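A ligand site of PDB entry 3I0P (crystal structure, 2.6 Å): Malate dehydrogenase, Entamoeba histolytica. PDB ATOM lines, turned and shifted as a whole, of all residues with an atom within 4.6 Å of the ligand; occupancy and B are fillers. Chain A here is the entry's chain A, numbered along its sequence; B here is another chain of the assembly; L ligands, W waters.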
ATOM      1  N   MET A  47      29.304 -24.773 -24.096  1.00  0.00           N
ATOM      2  CA  MET A  47      28.843 -25.375 -22.846  1.00  0.00           C
ATOM      3  C   MET A  47      30.052 -26.006 -22.172  1.00  0.00           C
ATOM      4  O   MET A  47      30.214 -27.215 -22.156  1.00  0.00           O
ATOM      5  CB  MET A  47      27.767 -26.444 -23.116  1.00  0.00           C
ATOM      6  CG  MET A  47      26.560 -25.982 -23.904  1.00  0.00           C
ATOM      7  SD  MET A  47      25.750 -24.629 -23.064  1.00  0.00           S
ATOM      8  CE  MET A  47      24.312 -24.368 -24.134  1.00  0.00           C
ATOM      9  N   HIS A  50      30.457 -29.386 -20.163  1.00  0.00           N
ATOM     10  CA  HIS A  50      29.913 -30.648 -20.671  1.00  0.00           C
ATOM     11  C   HIS A  50      30.704 -31.369 -21.760  1.00  0.00           C
ATOM     12  O   HIS A  50      30.220 -32.358 -22.338  1.00  0.00           O
ATOM     13  CB  HIS A  50      28.445 -30.472 -21.072  1.00  0.00           C
ATOM     14  CG  HIS A  50      27.517 -30.371 -19.902  1.00  0.00           C
ATOM     15  ND1 HIS A  50      27.056 -29.169 -19.415  1.00  0.00           N
ATOM     16  CD2 HIS A  50      26.992 -31.328 -19.106  1.00  0.00           C
ATOM     17  CE1 HIS A  50      26.276 -29.391 -18.376  1.00  0.00           C
ATOM     18  NE2 HIS A  50      26.217 -30.691 -18.160  1.00  0.00           N
ATOM     19  N   HIS A 123      24.881 -40.322 -17.868  1.00  0.00           N
ATOM     20  CA  HIS A 123      24.976 -38.922 -18.279  1.00  0.00           C
ATOM     21  C   HIS A 123      25.111 -38.783 -19.792  1.00  0.00           C
ATOM     22  O   HIS A 123      25.919 -39.473 -20.436  1.00  0.00           O
ATOM     23  CB  HIS A 123      26.153 -38.257 -17.577  1.00  0.00           C
ATOM     24  CG  HIS A 123      26.034 -36.773 -17.484  1.00  0.00           C
ATOM     25  ND1 HIS A 123      26.626 -35.918 -18.389  1.00  0.00           N
ATOM     26  CD2 HIS A 123      25.383 -35.981 -16.598  1.00  0.00           C
ATOM     27  CE1 HIS A 123      26.346 -34.671 -18.064  1.00  0.00           C
ATOM     28  NE2 HIS A 123      25.586 -34.685 -16.979  1.00  0.00           N
ATOM     29  N   PHE A 124      24.301 -37.903 -20.372  1.00  0.00           N
ATOM     30  CA  PHE A 124      24.239 -37.807 -21.829  1.00  0.00           C
ATOM     31  C   PHE A 124      24.711 -36.461 -22.376  1.00  0.00           C
ATOM     32  O   PHE A 124      24.435 -36.121 -23.520  1.00  0.00           O
ATOM     33  CB  PHE A 124      22.863 -38.274 -22.353  1.00  0.00           C
ATOM     34  CG  PHE A 124      21.766 -37.220 -22.355  1.00  0.00           C
ATOM     35  CD1 PHE A 124      20.541 -37.515 -22.938  1.00  0.00           C
ATOM     36  CD2 PHE A 124      21.963 -35.958 -21.806  1.00  0.00           C
ATOM     37  CE1 PHE A 124      19.523 -36.567 -22.967  1.00  0.00           C
ATOM     38  CE2 PHE A 124      20.947 -34.996 -21.845  1.00  0.00           C
ATOM     39  CZ  PHE A 124      19.720 -35.305 -22.418  1.00  0.00           C
ATOM     40  N   GLY A 125      25.441 -35.716 -21.548  1.00  0.00           N
ATOM     41  CA  GLY A 125      26.017 -34.443 -21.948  1.00  0.00           C
ATOM     42  C   GLY A 125      24.964 -33.399 -22.204  1.00  0.00           C
ATOM     43  O   GLY A 125      23.998 -33.287 -21.446  1.00  0.00           O
ATOM     44  N   ILE A 126      25.117 -32.627 -23.269  1.00  0.00           N
ATOM     45  CA  ILE A 126      24.173 -31.551 -23.554  1.00  0.00           C
ATOM     46  C   ILE A 126      22.860 -32.034 -24.181  1.00  0.00           C
ATOM     47  O   ILE A 126      22.860 -32.767 -25.176  1.00  0.00           O
ATOM     48  CB  ILE A 126      24.799 -30.405 -24.387  1.00  0.00           C
ATOM     49  CG1 ILE A 126      25.503 -30.924 -25.644  1.00  0.00           C
ATOM     50  CG2 ILE A 126      25.747 -29.619 -23.518  1.00  0.00           C
ATOM     51  CD1 ILE A 126      25.662 -29.858 -26.717  1.00  0.00           C
ATOM     52  N   ALA A 127      21.732 -31.617 -23.605  1.00  0.00           N
ATOM     53  CA  ALA A 127      20.437 -32.038 -24.139  1.00  0.00           C
ATOM     54  C   ALA A 127      20.292 -31.558 -25.580  1.00  0.00           C
ATOM     55  O   ALA A 127      19.784 -32.283 -26.441  1.00  0.00           O
ATOM     56  CB  ALA A 127      19.294 -31.530 -23.265  1.00  0.00           C
ATOM     57  N   GLY A 128      20.776 -30.339 -25.822  1.00  0.00           N
ATOM     58  CA  GLY A 128      20.693 -29.702 -27.131  1.00  0.00           C
ATOM     59  C   GLY A 128      21.212 -30.522 -28.274  1.00  0.00           C
ATOM     60  O   GLY A 128      20.788 -30.330 -29.413  1.00  0.00           O
ATOM     61  N   THR A 145      16.287 -35.248 -19.924  1.00  0.00           N
ATOM     62  CA  THR A 145      16.848 -36.289 -19.089  1.00  0.00           C
ATOM     63  C   THR A 145      16.547 -35.941 -17.646  1.00  0.00           C
ATOM     64  O   THR A 145      16.403 -34.769 -17.334  1.00  0.00           O
ATOM     65  CB  THR A 145      18.401 -36.425 -19.286  1.00  0.00           C
ATOM     66  OG1 THR A 145      18.890 -37.559 -18.568  1.00  0.00           O
ATOM     67  CG2 THR A 145      19.145 -35.183 -18.831  1.00  0.00           C
ATOM     68  N   ALA A 147      18.110 -36.309 -13.609  1.00  0.00           N
ATOM     69  CA  ALA A 147      19.436 -36.285 -13.004  1.00  0.00           C
ATOM     70  C   ALA A 147      19.287 -36.412 -11.499  1.00  0.00           C
ATOM     71  O   ALA A 147      18.174 -36.335 -10.981  1.00  0.00           O
ATOM     72  CB  ALA A 147      20.159 -34.995 -13.371  1.00  0.00           C
ATOM     73  N   THR A 163      18.302 -31.244 -12.196  1.00  0.00           N
ATOM     74  CA  THR A 163      18.267 -29.992 -12.923  1.00  0.00           C
ATOM     75  C   THR A 163      17.449 -30.176 -14.205  1.00  0.00           C
ATOM     76  O   THR A 163      17.063 -29.202 -14.861  1.00  0.00           O
ATOM     77  CB  THR A 163      19.674 -29.493 -13.242  1.00  0.00           C
ATOM     78  OG1 THR A 163      20.477 -30.602 -13.687  1.00  0.00           O
ATOM     79  CG2 THR A 163      20.310 -28.893 -12.001  1.00  0.00           C
ATOM     80  N   PRO A 165      17.116 -30.952 -17.639  1.00  0.00           N
ATOM     81  CA  PRO A 165      17.097 -30.045 -18.776  1.00  0.00           C
ATOM     82  C   PRO A 165      16.087 -30.470 -19.828  1.00  0.00           C
ATOM     83  O   PRO A 165      15.724 -31.655 -19.928  1.00  0.00           O
ATOM     84  CB  PRO A 165      18.524 -30.117 -19.317  1.00  0.00           C
ATOM     85  CG  PRO A 165      18.976 -31.479 -18.991  1.00  0.00           C
ATOM     86  CD  PRO A 165      18.299 -31.833 -17.670  1.00  0.00           C
ATOM     87  N   CYS A 179      17.470 -23.443 -31.216  1.00  0.00           N
ATOM     88  CA  CYS A 179      17.781 -24.493 -30.272  1.00  0.00           C
ATOM     89  C   CYS A 179      17.758 -23.989 -28.864  1.00  0.00           C
ATOM     90  O   CYS A 179      18.748 -23.426 -28.373  1.00  0.00           O
ATOM     91  CB  CYS A 179      19.149 -25.122 -30.558  1.00  0.00           C
ATOM     92  SG  CYS A 179      19.425 -26.595 -29.561  1.00  0.00           S
ATOM     93  N   PHE A 180      16.629 -24.192 -28.179  1.00  0.00           N
ATOM     94  CA  PHE A 180      16.632 -23.983 -26.748  1.00  0.00           C
ATOM     95  C   PHE A 180      17.229 -25.213 -26.076  1.00  0.00           C
ATOM     96  O   PHE A 180      16.937 -26.344 -26.464  1.00  0.00           O
ATOM     97  CB  PHE A 180      15.241 -23.682 -26.187  1.00  0.00           C
ATOM     98  CG  PHE A 180      15.245 -23.602 -24.686  1.00  0.00           C
ATOM     99  CD1 PHE A 180      15.902 -22.562 -24.043  1.00  0.00           C
ATOM    100  CD2 PHE A 180      14.659 -24.598 -23.917  1.00  0.00           C
ATOM    101  CE1 PHE A 180      15.941 -22.497 -22.669  1.00  0.00           C
ATOM    102  CE2 PHE A 180      14.682 -24.526 -22.527  1.00  0.00           C
ATOM    103  CZ  PHE A 180      15.324 -23.482 -21.903  1.00  0.00           C
ATOM    104  N   ASP A 181      18.091 -24.966 -25.095  1.00  0.00           N
ATOM    105  CA  ASP A 181      18.774 -26.039 -24.401  1.00  0.00           C
ATOM    106  C   ASP A 181      19.170 -25.573 -23.022  1.00  0.00           C
ATOM    107  O   ASP A 181      20.084 -24.768 -22.881  1.00  0.00           O
ATOM    108  CB  ASP A 181      20.007 -26.478 -25.203  1.00  0.00           C
ATOM    109  CG  ASP A 181      20.784 -27.566 -24.499  1.00  0.00           C
ATOM    110  OD1 ASP A 181      20.206 -28.281 -23.648  1.00  0.00           O
ATOM    111  OD2 ASP A 181      21.994 -27.703 -24.807  1.00  0.00           O
ATOM    112  N   GLY A 182      18.495 -26.070 -22.003  1.00  0.00           N
ATOM    113  CA  GLY A 182      18.766 -25.610 -20.658  1.00  0.00           C
ATOM    114  C   GLY A 182      18.040 -26.342 -19.555  1.00  0.00           C
ATOM    115  O   GLY A 182      17.018 -27.022 -19.803  1.00  0.00           O
ATOM    116  N   ALA A 183      18.571 -26.196 -18.335  1.00  0.00           N
ATOM    117  CA  ALA A 183      17.983 -26.794 -17.152  1.00  0.00           C
ATOM    118  C   ALA A 183      16.624 -26.190 -16.840  1.00  0.00           C
ATOM    119  O   ALA A 183      16.361 -25.042 -17.206  1.00  0.00           O
ATOM    120  CB  ALA A 183      18.904 -26.613 -15.978  1.00  0.00           C
ATOM    121  N   ILE A 186      16.995 -22.602 -12.542  1.00  0.00           N
ATOM    122  CA  ILE A 186      17.667 -21.398 -13.061  1.00  0.00           C
ATOM    123  C   ILE A 186      19.110 -21.736 -13.477  1.00  0.00           C
ATOM    124  O   ILE A 186      19.532 -21.404 -14.582  1.00  0.00           O
ATOM    125  CB  ILE A 186      17.649 -20.214 -12.046  1.00  0.00           C
ATOM    126  CG1 ILE A 186      16.199 -19.846 -11.679  1.00  0.00           C
ATOM    127  CG2 ILE A 186      18.409 -19.004 -12.624  1.00  0.00           C
ATOM    128  CD1 ILE A 186      16.052 -18.715 -10.654  1.00  0.00           C
ATOM    129  N   PRO A 188      22.263 -24.930 -13.520  1.00  0.00           N
ATOM    130  CA  PRO A 188      22.764 -26.296 -13.303  1.00  0.00           C
ATOM    131  C   PRO A 188      23.914 -26.341 -12.271  1.00  0.00           C
ATOM    132  O   PRO A 188      24.464 -25.300 -11.917  1.00  0.00           O
ATOM    133  CB  PRO A 188      23.257 -26.712 -14.691  1.00  0.00           C
ATOM    134  CG  PRO A 188      23.606 -25.438 -15.357  1.00  0.00           C
ATOM    135  CD  PRO A 188      22.648 -24.416 -14.846  1.00  0.00           C
ATOM    136  N   ARG A 191      27.567 -25.062 -13.483  1.00  0.00           N
ATOM    137  CA  ARG A 191      27.863 -23.625 -13.422  1.00  0.00           C
ATOM    138  C   ARG A 191      28.493 -23.273 -12.066  1.00  0.00           C
ATOM    139  O   ARG A 191      29.324 -22.362 -11.977  1.00  0.00           O
ATOM    140  CB  ARG A 191      26.588 -22.805 -13.671  1.00  0.00           C
ATOM    141  CG  ARG A 191      26.841 -21.382 -14.144  1.00  0.00           C
ATOM    142  CD  ARG A 191      25.562 -20.564 -14.187  1.00  0.00           C
ATOM    143  NE  ARG A 191      24.554 -21.131 -15.080  1.00  0.00           N
ATOM    144  CZ  ARG A 191      23.347 -20.614 -15.288  1.00  0.00           C
ATOM    145  NH1 ARG A 191      22.960 -19.510 -14.666  1.00  0.00           N
ATOM    146  NH2 ARG A 191      22.512 -21.210 -16.136  1.00  0.00           N
ATOM    147  N   TYR A 324      18.908 -11.790 -28.659  1.00  0.00           N
ATOM    148  CA  TYR A 324      19.284 -13.089 -29.213  1.00  0.00           C
ATOM    149  C   TYR A 324      18.062 -14.008 -29.356  1.00  0.00           C
ATOM    150  O   TYR A 324      16.990 -13.730 -28.816  1.00  0.00           O
ATOM    151  CB  TYR A 324      20.344 -13.771 -28.341  1.00  0.00           C
ATOM    152  CG  TYR A 324      21.595 -12.952 -28.082  1.00  0.00           C
ATOM    153  CD1 TYR A 324      22.800 -13.257 -28.716  1.00  0.00           C
ATOM    154  CD2 TYR A 324      21.564 -11.874 -27.190  1.00  0.00           C
ATOM    155  CE1 TYR A 324      23.941 -12.505 -28.482  1.00  0.00           C
ATOM    156  CE2 TYR A 324      22.714 -11.120 -26.942  1.00  0.00           C
ATOM    157  CZ  TYR A 324      23.899 -11.444 -27.594  1.00  0.00           C
ATOM    158  OH  TYR A 324      25.030 -10.700 -27.354  1.00  0.00           O
ATOM    159  N   THR A 325      18.234 -15.082 -30.108  1.00  0.00           N
ATOM    160  CA  THR A 325      17.254 -16.148 -30.117  1.00  0.00           C
ATOM    161  C   THR A 325      17.939 -17.476 -29.764  1.00  0.00           C
ATOM    162  O   THR A 325      19.170 -17.585 -29.811  1.00  0.00           O
ATOM    163  CB  THR A 325      16.495 -16.245 -31.463  1.00  0.00           C
ATOM    164  OG1 THR A 325      17.424 -16.568 -32.493  1.00  0.00           O
ATOM    165  CG2 THR A 325      15.786 -14.940 -31.804  1.00  0.00           C
ATOM    166  N   ALA A 326      17.137 -18.482 -29.387  1.00  0.00           N
ATOM    167  CA  ALA A 326      17.657 -19.776 -28.977  1.00  0.00           C
ATOM    168  C   ALA A 326      18.708 -20.293 -29.958  1.00  0.00           C
ATOM    169  O   ALA A 326      18.425 -20.439 -31.154  1.00  0.00           O
ATOM    170  CB  ALA A 326      16.527 -20.770 -28.836  1.00  0.00           C
ATOM    171  N   GLY A 327      19.909 -20.540 -29.454  1.00  0.00           N
ATOM    172  CA  GLY A 327      20.966 -21.146 -30.253  1.00  0.00           C
ATOM    173  C   GLY A 327      21.883 -20.195 -30.993  1.00  0.00           C
ATOM    174  O   GLY A 327      22.810 -20.635 -31.670  1.00  0.00           O
ATOM    175  N   GLU A 328      21.637 -18.891 -30.874  1.00  0.00           N
ATOM    176  CA  GLU A 328      22.414 -17.856 -31.581  1.00  0.00           C
ATOM    177  C   GLU A 328      23.797 -17.715 -30.955  1.00  0.00           C
ATOM    178  O   GLU A 328      24.813 -17.801 -31.658  1.00  0.00           O
ATOM    179  CB  GLU A 328      21.672 -16.501 -31.566  1.00  0.00           C
ATOM    180  CG  GLU A 328      22.271 -15.422 -32.453  1.00  0.00           C
ATOM    181  CD  GLU A 328      21.357 -14.205 -32.598  1.00  0.00           C
ATOM    182  OE1 GLU A 328      20.337 -14.146 -31.873  1.00  0.00           O
ATOM    183  OE2 GLU A 328      21.640 -13.317 -33.455  1.00  0.00           O
ATOM    184  N   LYS A 329      23.823 -17.492 -29.635  1.00  0.00           N
ATOM    185  CA  LYS A 329      25.041 -17.471 -28.837  1.00  0.00           C
ATOM    186  C   LYS A 329      25.912 -18.722 -29.061  1.00  0.00           C
ATOM    187  O   LYS A 329      27.144 -18.619 -29.071  1.00  0.00           O
ATOM    188  CB  LYS A 329      24.704 -17.296 -27.349  1.00  0.00           C
ATOM    189  CG  LYS A 329      24.764 -15.859 -26.879  1.00  0.00           C
ATOM    190  CD  LYS A 329      23.704 -15.525 -25.841  1.00  0.00           C
ATOM    191  CE  LYS A 329      24.231 -15.589 -24.419  1.00  0.00           C
ATOM    192  NZ  LYS A 329      23.521 -14.568 -23.599  1.00  0.00           N
ATOM    193  N   GLU A 330      25.278 -19.873 -29.251  1.00  0.00           N
ATOM    194  CA  GLU A 330      26.023 -21.109 -29.444  1.00  0.00           C
ATOM    195  C   GLU A 330      26.648 -21.162 -30.818  1.00  0.00           C
ATOM    196  O   GLU A 330      27.753 -21.677 -30.963  1.00  0.00           O
ATOM    197  CB  GLU A 330      25.154 -22.330 -29.200  1.00  0.00           C
ATOM    198  CG  GLU A 330      24.884 -22.618 -27.710  1.00  0.00           C
ATOM    199  CD  GLU A 330      23.796 -21.742 -27.110  1.00  0.00           C
ATOM    200  OE1 GLU A 330      22.940 -21.228 -27.863  1.00  0.00           O
ATOM    201  OE2 GLU A 330      23.785 -21.568 -25.882  1.00  0.00           O
ATOM    202  N   THR B 154      13.850 -11.083 -24.241  1.00  0.00           N
ATOM    203  CA  THR B 154      14.959 -10.759 -23.338  1.00  0.00           C
ATOM    204  C   THR B 154      15.808  -9.665 -23.982  1.00  0.00           C
ATOM    205  O   THR B 154      16.252  -9.793 -25.127  1.00  0.00           O
ATOM    206  CB  THR B 154      15.829 -11.993 -23.015  1.00  0.00           C
ATOM    207  OG1 THR B 154      15.001 -13.028 -22.462  1.00  0.00           O
ATOM    208  CG2 THR B 154      16.908 -11.649 -22.017  1.00  0.00           C
ATOM    209  N   PHE B 155      16.002  -8.577 -23.231  1.00  0.00           N
ATOM    210  CA  PHE B 155      16.673  -7.331 -23.674  1.00  0.00           C
ATOM    211  C   PHE B 155      15.749  -6.441 -24.514  1.00  0.00           C
ATOM    212  O   PHE B 155      16.214  -5.477 -25.140  1.00  0.00           O
ATOM    213  CB  PHE B 155      18.003  -7.601 -24.428  1.00  0.00           C
ATOM    214  CG  PHE B 155      18.972  -8.464 -23.668  1.00  0.00           C
ATOM    215  CD1 PHE B 155      19.116  -8.362 -22.280  1.00  0.00           C
ATOM    216  CD2 PHE B 155      19.776  -9.388 -24.350  1.00  0.00           C
ATOM    217  CE1 PHE B 155      20.024  -9.168 -21.581  1.00  0.00           C
ATOM    218  CE2 PHE B 155      20.688 -10.202 -23.672  1.00  0.00           C
ATOM    219  CZ  PHE B 155      20.807 -10.096 -22.284  1.00  0.00           C
ATOM    220  N   GLU B 240      19.005 -12.296 -17.534  1.00  0.00           N
ATOM    221  CA  GLU B 240      19.479 -13.654 -17.790  1.00  0.00           C
ATOM    222  C   GLU B 240      19.847 -14.346 -16.482  1.00  0.00           C
ATOM    223  O   GLU B 240      19.743 -15.566 -16.355  1.00  0.00           O
ATOM    224  CB  GLU B 240      20.710 -13.636 -18.685  1.00  0.00           C
ATOM    225  CG  GLU B 240      20.430 -13.221 -20.097  1.00  0.00           C
ATOM    226  CD  GLU B 240      21.685 -13.209 -20.938  1.00  0.00           C
ATOM    227  OE1 GLU B 240      22.787 -13.089 -20.360  1.00  0.00           O
ATOM    228  OE2 GLU B 240      21.562 -13.316 -22.174  1.00  0.00           O
ATOM    229  N   HIS B 245      15.914 -15.589 -20.265  1.00  0.00           N
ATOM    230  CA  HIS B 245      16.109 -16.183 -21.583  1.00  0.00           C
ATOM    231  C   HIS B 245      15.353 -17.501 -21.767  1.00  0.00           C
ATOM    232  O   HIS B 245      14.936 -17.837 -22.885  1.00  0.00           O
ATOM    233  CB  HIS B 245      17.593 -16.368 -21.887  1.00  0.00           C
ATOM    234  CG  HIS B 245      18.349 -17.139 -20.841  1.00  0.00           C
ATOM    235  ND1 HIS B 245      18.518 -16.670 -19.553  1.00  0.00           N
ATOM    236  CD2 HIS B 245      18.987 -18.327 -20.898  1.00  0.00           C
ATOM    237  CE1 HIS B 245      19.216 -17.555 -18.859  1.00  0.00           C
ATOM    238  NE2 HIS B 245      19.510 -18.566 -19.646  1.00  0.00           N
ATOM    239  N   LYS B 246      15.159 -18.218 -20.667  1.00  0.00           N
ATOM    240  CA  LYS B 246      14.460 -19.487 -20.717  1.00  0.00           C
ATOM    241  C   LYS B 246      12.948 -19.303 -20.985  1.00  0.00           C
ATOM    242  O   LYS B 246      12.436 -19.819 -21.975  1.00  0.00           O
ATOM    243  CB  LYS B 246      14.759 -20.329 -19.458  1.00  0.00           C
ATOM    244  CG  LYS B 246      16.242 -20.674 -19.340  1.00  0.00           C
ATOM    245  CD  LYS B 246      16.564 -21.443 -18.094  1.00  0.00           C
ATOM    246  CE  LYS B 246      18.008 -21.930 -18.131  1.00  0.00           C
ATOM    247  NZ  LYS B 246      18.267 -22.997 -17.134  1.00  0.00           N
ATOM    248  N   TYR B 248      11.483 -16.752 -22.125  1.00  0.00           N
ATOM    249  CA  TYR B 248      11.459 -16.137 -23.451  1.00  0.00           C
ATOM    250  C   TYR B 248      11.569 -17.182 -24.572  1.00  0.00           C
ATOM    251  O   TYR B 248      10.746 -17.189 -25.489  1.00  0.00           O
ATOM    252  CB  TYR B 248      12.545 -15.057 -23.527  1.00  0.00           C
ATOM    253  CG  TYR B 248      12.960 -14.609 -24.913  1.00  0.00           C
ATOM    254  CD1 TYR B 248      12.016 -14.317 -25.907  1.00  0.00           C
ATOM    255  CD2 TYR B 248      14.314 -14.447 -25.222  1.00  0.00           C
ATOM    256  CE1 TYR B 248      12.405 -13.906 -27.183  1.00  0.00           C
ATOM    257  CE2 TYR B 248      14.720 -14.003 -26.481  1.00  0.00           C
ATOM    258  CZ  TYR B 248      13.759 -13.740 -27.458  1.00  0.00           C
ATOM    259  OH  TYR B 248      14.172 -13.330 -28.701  1.00  0.00           O
ATOM    260  N   CYS B 249      12.556 -18.072 -24.493  1.00  0.00           N
ATOM    261  CA  CYS B 249      12.689 -19.159 -25.471  1.00  0.00           C
ATOM    262  C   CYS B 249      11.485 -20.099 -25.485  1.00  0.00           C
ATOM    263  O   CYS B 249      11.067 -20.545 -26.556  1.00  0.00           O
ATOM    264  CB  CYS B 249      13.976 -19.952 -25.261  1.00  0.00           C
ATOM    265  SG  CYS B 249      15.445 -18.988 -25.677  1.00  0.00           S
HETATM  266  P1  LIG L   1      21.658 -21.428 -20.031  1.00  0.00           P
HETATM  267  O1  LIG L   1      23.104 -21.254 -20.430  1.00  0.00           O
HETATM  268  O2  LIG L   1      21.144 -20.627 -18.875  1.00  0.00           O
HETATM  269  O3  LIG L   1      20.787 -21.113 -21.343  1.00  0.00           O
HETATM  270  C1  LIG L   1      21.110 -21.762 -22.590  1.00  0.00           C
HETATM  271  C2  LIG L   1      19.984 -21.620 -23.626  1.00  0.00           C
HETATM  272  O4  LIG L   1      19.363 -20.331 -23.577  1.00  0.00           O
HETATM  273  C3  LIG L   1      20.487 -21.766 -25.041  1.00  0.00           C
HETATM  274  O5  LIG L   1      19.438 -22.330 -25.843  1.00  0.00           O
HETATM  275  C4  LIG L   1      20.753 -20.337 -25.475  1.00  0.00           C
HETATM  276  O6  LIG L   1      20.674 -20.190 -26.897  1.00  0.00           O
HETATM  277  C5  LIG L   1      19.634 -19.600 -24.785  1.00  0.00           C
HETATM  278  N1  LIG L   1      19.928 -18.173 -24.451  1.00  0.00           N
HETATM  279  C6  LIG L   1      20.878 -17.707 -23.635  1.00  0.00           C
HETATM  280  N2  LIG L   1      20.786 -16.366 -23.579  1.00  0.00           N
HETATM  281  C7  LIG L   1      19.764 -15.988 -24.380  1.00  0.00           C
HETATM  282  C8  LIG L   1      19.191 -14.759 -24.734  1.00  0.00           C
HETATM  283  N3  LIG L   1      19.679 -13.591 -24.237  1.00  0.00           N
HETATM  284  N4  LIG L   1      18.144 -14.719 -25.589  1.00  0.00           N
HETATM  285  C9  LIG L   1      17.632 -15.855 -26.097  1.00  0.00           C
HETATM  286  N5  LIG L   1      18.165 -17.049 -25.773  1.00  0.00           N
HETATM  287  C10 LIG L   1      19.222 -17.132 -24.924  1.00  0.00           C
HETATM  288  O7  LIG L   1      21.303 -23.002 -19.796  1.00  0.00           O
HETATM  289  P2  LIG L   1      21.800 -23.996 -18.607  1.00  0.00           P
HETATM  290  O8  LIG L   1      20.573 -24.373 -17.806  1.00  0.00           O
HETATM  291  O9  LIG L   1      23.019 -23.427 -17.926  1.00  0.00           O
HETATM  292  O10 LIG L   1      22.282 -25.303 -19.398  1.00  0.00           O
HETATM  293  C11 LIG L   1      23.581 -25.356 -20.009  1.00  0.00           C
HETATM  294  C12 LIG L   1      23.853 -26.762 -20.551  1.00  0.00           C
HETATM  295  O11 LIG L   1      23.883 -27.709 -19.475  1.00  0.00           O
HETATM  296  C13 LIG L   1      22.761 -27.232 -21.507  1.00  0.00           C
HETATM  297  O12 LIG L   1      23.389 -27.608 -22.737  1.00  0.00           O
HETATM  298  C14 LIG L   1      22.085 -28.410 -20.794  1.00  0.00           C
HETATM  299  O13 LIG L   1      21.661 -29.489 -21.649  1.00  0.00           O
HETATM  300  C15 LIG L   1      23.190 -28.888 -19.876  1.00  0.00           C
HETATM  301  N6  LIG L   1      22.663 -29.648 -18.749  1.00  0.00           N
HETATM  302  C16 LIG L   1      22.754 -30.994 -18.782  1.00  0.00           C
HETATM  303  C17 LIG L   1      22.267 -31.762 -17.724  1.00  0.00           C
HETATM  304  C18 LIG L   1      22.362 -33.263 -17.739  1.00  0.00           C
HETATM  305  O14 LIG L   1      21.928 -33.904 -16.783  1.00  0.00           O
HETATM  306  N7  LIG L   1      22.923 -33.867 -18.783  1.00  0.00           N
HETATM  307  C19 LIG L   1      21.682 -31.120 -16.627  1.00  0.00           C
HETATM  308  C20 LIG L   1      21.586 -29.727 -16.619  1.00  0.00           C
HETATM  309  C21 LIG L   1      22.091 -29.002 -17.701  1.00  0.00           C
HETATM  310  O   HOH W   1      21.463 -17.375 -27.890  1.00  0.00           O
HETATM  311  O   HOH W   2      25.638 -22.920 -17.109  1.00  0.00           O
HETATM  312  O   HOH W   3      21.375 -24.243 -27.923  1.00  0.00           O
HETATM  313  O   HOH W   4      22.085 -36.885 -18.342  1.00  0.00           O
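OE1 of Glu 330 is in hydrogen-bond range of O6 of the ligand.
An oxygen (O9) of the ligand is in salt-bridge range of the guanidinium group (NH2) of Arg 191, 2.9 Å away.
O13 of the ligand lies within hydrogen-bond range of N of Ala 127 (2.9 Å).
O2 of the ligand is in hydrogen-bond range of NE2 of His 245 of chain B (2.7 Å).
An oxygen (O5) of the ligand lies within hydrogen-bond range of the backbone NH (N) of Asp 181.
A nitrogen (N7) of the ligand lies within hydrogen-bond range of the backbone carbonyl oxygen (O) of Gly 125 (2.9 Å).
NE2 of His 123 lies within hydrogen-bond range of N7 of the ligand (3.3 Å).
The backbone NH (N) of Gly 327 sits at hydrogen-bond distance from an oxygen (O6) of the ligand (2.7 Å).
N5 of the ligand is in hydrogen-bond range of SG of Cys 249 of chain B (3.3 Å).
The backbone carbonyl oxygen (O) of Cys 179 sits at hydrogen-bond distance from an oxygen (O5) of the ligand.
A ring nitrogen (ND1) of His 50 lies close to an oxygen (O11) of the ligand.
An oxygen (O8) of the ligand sits at hydrogen-bond distance from the backbone NH of Ala 183 (2.8 Å).
The side-chain amino group of Lys 329 sits at hydrogen-bond distance from a nitrogen (N2) of the ligand, at 3.3 Å.
An oxygen (O12) of the ligand is in hydrogen-bond range of the side-chain carboxylate of Asp 181 (2.5 Å).
O8 of the ligand is in salt-bridge range of NZ of Lys 246 of chain B.
The side-chain carboxylate (OE2) of Glu 240 of chain B sits at hydrogen-bond distance from a nitrogen (N3) of the ligand (2.8 Å).
Residues that only touch the ligand: Ile 126, Thr 163, Pro 188, Phe 180, Tyr 248 of chain B, Tyr 324, Pro 165, Phe 155 of chain B, Gly 182, Ala 326, Met 47, Thr 145, Phe 124 and Ala 147.
Hydrophobic or aromatic side chains that line the ligand: Met 47, His 50, His 123, Phe 124, Ile 126, Ala 127, Ala 147, Pro 165, Phe 180, Ala 183, Pro 188, Tyr 324, Phe 155 of chain B, His 245 of chain B and Tyr 248 of chain B.
Along chain A the residues within 4 Å of the ligand span positions 47 to 330.
The side-chain carboxylate of Asp 181 is in hydrogen-bond range of the backbone NH of Gly 128, at 3.0 Å.
N of His 245 of chain B sits close to OG1 of Thr 154 of chain B.
The side-chain carboxylate (OE1) of Glu 330 sits close to the backbone NH (N) of Gly 327, at 3.5 Å.
The side-chain amino group (NZ) of Lys 246 of chain B is in hydrogen-bond range of the backbone carbonyl oxygen (O) of Ile 186 (3.3 Å).
O of His 245 of chain B lies within hydrogen-bond range of SG of Cys 249 of chain B (3.1 Å).
The side-chain hydroxyl (OH) of Tyr 248 of chain B sits at hydrogen-bond distance from the backbone carbonyl oxygen (O) of Tyr 324, at 2.8 Å.
The backbone NH (N) of Gly 125 sits at hydrogen-bond distance from a ring nitrogen (ND1) of His 123, 3.4 Å away.
OE2 of Glu 240 of chain B is in salt-bridge range of NZ of Lys 329, at 2.7 Å.
Water W2 bridges an oxygen (O9) of the ligand (2.8 Å) and the guanidinium group of Arg 191 (2.9 Å).
Water W1 lies within hydrogen-bond range of the backbone NH of Lys 329 (2.9 Å), the backbone carbonyl oxygen of Thr 325 (3.0 Å), an oxygen (O6) of the ligand (3.1 Å) and the backbone NH of Glu 328 (3.4 Å).
Water W4 lies within hydrogen-bond range of a nitrogen (N7) of the ligand (3.2 Å), the backbone NH of Phe 124 (3.2 Å) and the side-chain hydroxyl of Thr 145 (3.3 Å).
Water W3 lies within hydrogen-bond range of the backbone carbonyl oxygen (O) of Cys 179 (2.8 Å), the side-chain carboxylate (OE1) of Glu 330 (3.4 Å) and an oxygen (O5) of the ligand (3.4 Å).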
